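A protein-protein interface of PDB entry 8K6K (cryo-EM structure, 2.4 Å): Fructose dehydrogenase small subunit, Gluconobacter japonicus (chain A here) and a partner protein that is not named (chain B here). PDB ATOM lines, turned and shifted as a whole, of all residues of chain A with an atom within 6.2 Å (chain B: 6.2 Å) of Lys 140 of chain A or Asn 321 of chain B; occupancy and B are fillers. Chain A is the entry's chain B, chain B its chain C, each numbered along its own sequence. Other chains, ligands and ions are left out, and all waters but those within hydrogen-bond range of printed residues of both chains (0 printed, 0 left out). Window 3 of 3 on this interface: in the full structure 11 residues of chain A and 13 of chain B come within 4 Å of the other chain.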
ATOM      1  N   GLY A 131      11.551  14.121  20.645  1.00  0.00           N
ATOM      2  CA  GLY A 131      10.851  15.278  21.152  1.00  0.00           C
ATOM      3  C   GLY A 131       9.922  15.952  20.171  1.00  0.00           C
ATOM      4  O   GLY A 131       9.386  17.020  20.486  1.00  0.00           O
ATOM      5  N   VAL A 132       9.718  15.370  18.990  1.00  0.00           N
ATOM      6  CA  VAL A 132       8.796  15.900  17.999  1.00  0.00           C
ATOM      7  C   VAL A 132       7.869  14.782  17.547  1.00  0.00           C
ATOM      8  O   VAL A 132       8.191  13.596  17.643  1.00  0.00           O
ATOM      9  CB  VAL A 132       9.518  16.512  16.780  1.00  0.00           C
ATOM     10  CG1 VAL A 132      10.194  17.807  17.162  1.00  0.00           C
ATOM     11  CG2 VAL A 132      10.523  15.530  16.211  1.00  0.00           C
ATOM     12  N   ILE A 133       6.705  15.178  17.045  1.00  0.00           N
ATOM     13  CA  ILE A 133       5.723  14.249  16.514  1.00  0.00           C
ATOM     14  C   ILE A 133       5.602  14.367  15.000  1.00  0.00           C
ATOM     15  O   ILE A 133       5.557  13.355  14.297  1.00  0.00           O
ATOM     16  CB  ILE A 133       4.355  14.460  17.198  1.00  0.00           C
ATOM     17  CG1 ILE A 133       4.389  13.899  18.616  1.00  0.00           C
ATOM     18  CG2 ILE A 133       3.248  13.801  16.404  1.00  0.00           C
ATOM     19  CD1 ILE A 133       3.592  14.698  19.596  1.00  0.00           C
ATOM     20  N   GLU A 134       5.567  15.588  14.481  1.00  0.00           N
ATOM     21  CA  GLU A 134       5.521  15.816  13.045  1.00  0.00           C
ATOM     22  C   GLU A 134       6.934  15.703  12.473  1.00  0.00           C
ATOM     23  O   GLU A 134       7.881  15.327  13.166  1.00  0.00           O
ATOM     24  CB  GLU A 134       4.876  17.167  12.754  1.00  0.00           C
ATOM     25  CG  GLU A 134       3.753  17.540  13.701  1.00  0.00           C
ATOM     26  CD  GLU A 134       2.394  17.106  13.191  1.00  0.00           C
ATOM     27  OE1 GLU A 134       2.308  16.030  12.563  1.00  0.00           O
ATOM     28  OE2 GLU A 134       1.411  17.841  13.419  1.00  0.00           O
ATOM     29  N   ASN A 138       8.542  23.529  11.072  1.00  0.00           N
ATOM     30  CA  ASN A 138       7.809  24.203  12.133  1.00  0.00           C
ATOM     31  C   ASN A 138       7.133  23.222  13.082  1.00  0.00           C
ATOM     32  O   ASN A 138       6.165  23.587  13.756  1.00  0.00           O
ATOM     33  CB  ASN A 138       6.781  25.170  11.546  1.00  0.00           C
ATOM     34  CG  ASN A 138       6.019  24.576  10.384  1.00  0.00           C
ATOM     35  OD1 ASN A 138       6.514  23.689   9.693  1.00  0.00           O
ATOM     36  ND2 ASN A 138       4.804  25.063  10.162  1.00  0.00           N
ATOM     37  N   ALA A 139       7.616  21.983  13.138  1.00  0.00           N
ATOM     38  CA  ALA A 139       7.079  21.017  14.083  1.00  0.00           C
ATOM     39  C   ALA A 139       7.375  21.456  15.509  1.00  0.00           C
ATOM     40  O   ALA A 139       8.449  21.982  15.806  1.00  0.00           O
ATOM     41  CB  ALA A 139       7.671  19.634  13.822  1.00  0.00           C
ATOM     42  N   LYS A 140       6.407  21.244  16.394  1.00  0.00           N
ATOM     43  CA  LYS A 140       6.576  21.629  17.786  1.00  0.00           C
ATOM     44  C   LYS A 140       7.539  20.683  18.491  1.00  0.00           C
ATOM     45  O   LYS A 140       7.458  19.462  18.341  1.00  0.00           O
ATOM     46  CB  LYS A 140       5.228  21.637  18.501  1.00  0.00           C
ATOM     47  CG  LYS A 140       4.542  22.988  18.496  1.00  0.00           C
ATOM     48  CD  LYS A 140       3.045  22.848  18.324  1.00  0.00           C
ATOM     49  CE  LYS A 140       2.304  23.909  19.115  1.00  0.00           C
ATOM     50  NZ  LYS A 140       2.258  23.583  20.567  1.00  0.00           N
ATOM     51  N   VAL A 141       8.457  21.256  19.262  1.00  0.00           N
ATOM     52  CA  VAL A 141       9.422  20.495  20.044  1.00  0.00           C
ATOM     53  C   VAL A 141       8.918  20.432  21.477  1.00  0.00           C
ATOM     54  O   VAL A 141       8.667  21.469  22.102  1.00  0.00           O
ATOM     55  CB  VAL A 141      10.824  21.120  19.975  1.00  0.00           C
ATOM     56  CG1 VAL A 141      11.697  20.585  21.092  1.00  0.00           C
ATOM     57  CG2 VAL A 141      11.458  20.837  18.632  1.00  0.00           C
ATOM     58  N   TYR A 142       8.758  19.217  21.997  1.00  0.00           N
ATOM     59  CA  TYR A 142       8.240  19.016  23.339  1.00  0.00           C
ATOM     60  C   TYR A 142       9.303  18.603  24.343  1.00  0.00           C
ATOM     61  O   TYR A 142       9.015  18.578  25.544  1.00  0.00           O
ATOM     62  CB  TYR A 142       7.118  17.968  23.319  1.00  0.00           C
ATOM     63  CG  TYR A 142       5.975  18.355  22.414  1.00  0.00           C
ATOM     64  CD1 TYR A 142       5.008  19.253  22.835  1.00  0.00           C
ATOM     65  CD2 TYR A 142       5.876  17.841  21.132  1.00  0.00           C
ATOM     66  CE1 TYR A 142       3.969  19.618  22.011  1.00  0.00           C
ATOM     67  CE2 TYR A 142       4.838  18.200  20.301  1.00  0.00           C
ATOM     68  CZ  TYR A 142       3.889  19.089  20.745  1.00  0.00           C
ATOM     69  OH  TYR A 142       2.853  19.454  19.921  1.00  0.00           O
ATOM     70  N   VAL B 317       9.317  23.052  27.774  1.00  0.00           N
ATOM     71  CA  VAL B 317       9.826  23.220  26.417  1.00  0.00           C
ATOM     72  C   VAL B 317       8.678  23.450  25.445  1.00  0.00           C
ATOM     73  O   VAL B 317       8.800  24.223  24.489  1.00  0.00           O
ATOM     74  CB  VAL B 317      10.677  22.003  26.011  1.00  0.00           C
ATOM     75  CG1 VAL B 317      11.369  22.256  24.688  1.00  0.00           C
ATOM     76  CG2 VAL B 317      11.693  21.689  27.090  1.00  0.00           C
ATOM     77  N   ALA B 318       7.543  22.784  25.676  1.00  0.00           N
ATOM     78  CA  ALA B 318       6.410  22.899  24.765  1.00  0.00           C
ATOM     79  C   ALA B 318       5.871  24.322  24.720  1.00  0.00           C
ATOM     80  O   ALA B 318       5.457  24.804  23.660  1.00  0.00           O
ATOM     81  CB  ALA B 318       5.311  21.922  25.177  1.00  0.00           C
ATOM     82  N   ASN B 319       5.862  25.012  25.862  1.00  0.00           N
ATOM     83  CA  ASN B 319       5.348  26.375  25.905  1.00  0.00           C
ATOM     84  C   ASN B 319       6.215  27.352  25.123  1.00  0.00           C
ATOM     85  O   ASN B 319       5.745  28.443  24.788  1.00  0.00           O
ATOM     86  CB  ASN B 319       5.223  26.843  27.353  1.00  0.00           C
ATOM     87  CG  ASN B 319       4.123  26.124  28.103  1.00  0.00           C
ATOM     88  OD1 ASN B 319       3.367  25.347  27.522  1.00  0.00           O
ATOM     89  ND2 ASN B 319       4.028  26.379  29.401  1.00  0.00           N
ATOM     90  N   ALA B 320       7.464  26.992  24.831  1.00  0.00           N
ATOM     91  CA  ALA B 320       8.360  27.881  24.107  1.00  0.00           C
ATOM     92  C   ALA B 320       8.141  27.856  22.602  1.00  0.00           C
ATOM     93  O   ALA B 320       8.697  28.706  21.900  1.00  0.00           O
ATOM     94  CB  ALA B 320       9.815  27.522  24.414  1.00  0.00           C
ATOM     95  N   ASN B 321       7.352  26.908  22.094  1.00  0.00           N
ATOM     96  CA  ASN B 321       7.135  26.816  20.654  1.00  0.00           C
ATOM     97  C   ASN B 321       6.407  28.044  20.125  1.00  0.00           C
ATOM     98  O   ASN B 321       6.689  28.510  19.015  1.00  0.00           O
ATOM     99  CB  ASN B 321       6.354  25.548  20.327  1.00  0.00           C
ATOM    100  CG  ASN B 321       7.150  24.295  20.591  1.00  0.00           C
ATOM    101  OD1 ASN B 321       8.269  24.144  20.106  1.00  0.00           O
ATOM    102  ND2 ASN B 321       6.580  23.384  21.366  1.00  0.00           N
ATOM    103  N   SER B 322       5.461  28.576  20.899  1.00  0.00           N
ATOM    104  CA  SER B 322       4.759  29.785  20.494  1.00  0.00           C
ATOM    105  C   SER B 322       5.684  30.991  20.418  1.00  0.00           C
ATOM    106  O   SER B 322       5.371  31.952  19.708  1.00  0.00           O
ATOM    107  CB  SER B 322       3.613  30.073  21.462  1.00  0.00           C
ATOM    108  OG  SER B 322       4.109  30.392  22.748  1.00  0.00           O
ATOM    109  N   ARG B 323       6.809  30.962  21.124  1.00  0.00           N
ATOM    110  CA  ARG B 323       7.746  32.074  21.145  1.00  0.00           C
ATOM    111  C   ARG B 323       8.829  31.950  20.085  1.00  0.00           C
ATOM    112  O   ARG B 323       9.767  32.751  20.080  1.00  0.00           O
ATOM    113  CB  ARG B 323       8.379  32.205  22.530  1.00  0.00           C
ATOM    114  CG  ARG B 323       7.527  32.984  23.511  1.00  0.00           C
ATOM    115  CD  ARG B 323       8.248  33.209  24.821  1.00  0.00           C
ATOM    116  NE  ARG B 323       8.978  32.025  25.258  1.00  0.00           N
ATOM    117  CZ  ARG B 323       8.492  31.112  26.085  1.00  0.00           C
ATOM    118  NH1 ARG B 323       7.265  31.200  26.566  1.00  0.00           N
ATOM    119  NH2 ARG B 323       9.259  30.086  26.441  1.00  0.00           N
ATOM    120  N   ARG B 324       8.742  30.956  19.210  1.00  0.00           N
ATOM    121  CA  ARG B 324       9.598  30.948  18.037  1.00  0.00           C
ATOM    122  C   ARG B 324       9.143  32.038  17.073  1.00  0.00           C
ATOM    123  O   ARG B 324       7.999  32.500  17.114  1.00  0.00           O
ATOM    124  CB  ARG B 324       9.579  29.579  17.361  1.00  0.00           C
ATOM    125  CG  ARG B 324      10.113  28.462  18.240  1.00  0.00           C
ATOM    126  CD  ARG B 324      10.096  27.126  17.527  1.00  0.00           C
ATOM    127  NE  ARG B 324       8.747  26.712  17.168  1.00  0.00           N
ATOM    128  CZ  ARG B 324       8.431  25.509  16.708  1.00  0.00           C
ATOM    129  NH1 ARG B 324       9.347  24.569  16.546  1.00  0.00           N
ATOM    130  NH2 ARG B 324       7.165  25.243  16.404  1.00  0.00           N
ATOM    131  N   SER B 325      10.062  32.462  16.208  1.00  0.00           N
ATOM    132  CA  SER B 325       9.841  33.609  15.329  1.00  0.00           C
ATOM    133  C   SER B 325       9.545  34.874  16.129  1.00  0.00           C
ATOM    134  O   SER B 325       8.775  35.732  15.693  1.00  0.00           O
ATOM    135  CB  SER B 325       8.719  33.340  14.322  1.00  0.00           C
ATOM    136  OG  SER B 325       7.454  33.609  14.900  1.00  0.00           O
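Gly 131 of chain A touches none of the printed residues of chain B.
Lys 140 of chain A touches just these residues of chain B: Asn 321 and Arg 324.
Printed residues of chain B within 4 Å of Val 141 of chain A: Val 317, Ala 318 and Asn 321.
Of the printed residues of chain A, Val 317 of chain B touches Val 141 and Tyr 142.
Asn 321 of chain B touches just these residues of chain A: Lys 140 and Val 141.
Arg 323 of chain B touches none of the printed residues of chain A.
N of Tyr 142 of chain A is in hydrogen-bond range of O of Gly 131 of chain A (2.7 Å).
The side-chain amide nitrogen of Asn 321 of chain B lies within hydrogen-bond range of the backbone carbonyl oxygen of Ala 318 of chain B (2.9 Å).
The backbone carbonyl oxygen (O) of Asn 321 of chain B lies within hydrogen-bond range of the guanidinium group (NE) of Arg 324 of chain B, at 3.3 Å.
Of the 9 printed residues of chain B, 4 touch a printed residue of chain A.
Printed residues of chain B that touch a printed residue of chain A: Val 317, Ala 318, Asn 321 and Arg 324.
Hydrophobic or aromatic side chains of chain B within 4 Å of the printed part of chain A: Val 317 and Ala 318.
Among the printed residues, 9 pairs touch across the chains.
Among the printed residues, no Asp or Glu carboxylate lies within 4 Å of a Lys or Arg side-chain nitrogen of the other chain.
The backbone carbonyl oxygen (O) of Asn 138 of chain A lies within hydrogen-bond range of the guanidinium group (NH2) of Arg 324 of chain B (3.3 Å).
NH1 of Arg 324 of chain B sits at hydrogen-bond distance from O of Ala 139 of chain A (2.8 Å).
The side-chain amide nitrogen of Asn 321 of chain B sits at hydrogen-bond distance from the backbone carbonyl oxygen of Val 141 of chain A (2.9 Å).
Among the printed residues, merely in contact across the chains: Lys 140 of chain A with Asn 321 of chain B (3.5 Å), Lys 140 of chain A with Arg 324 of chain B (3.9 Å), Val 141 of chain A with Val 317 of chain B (3.6 Å), Val 141 of chain A with Ala 318 of chain B (3.8 Å), Tyr 142 of chain A with Val 317 of chain B (3.8 Å) and Tyr 142 of chain A with Ala 318 of chain B (3.6 Å).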
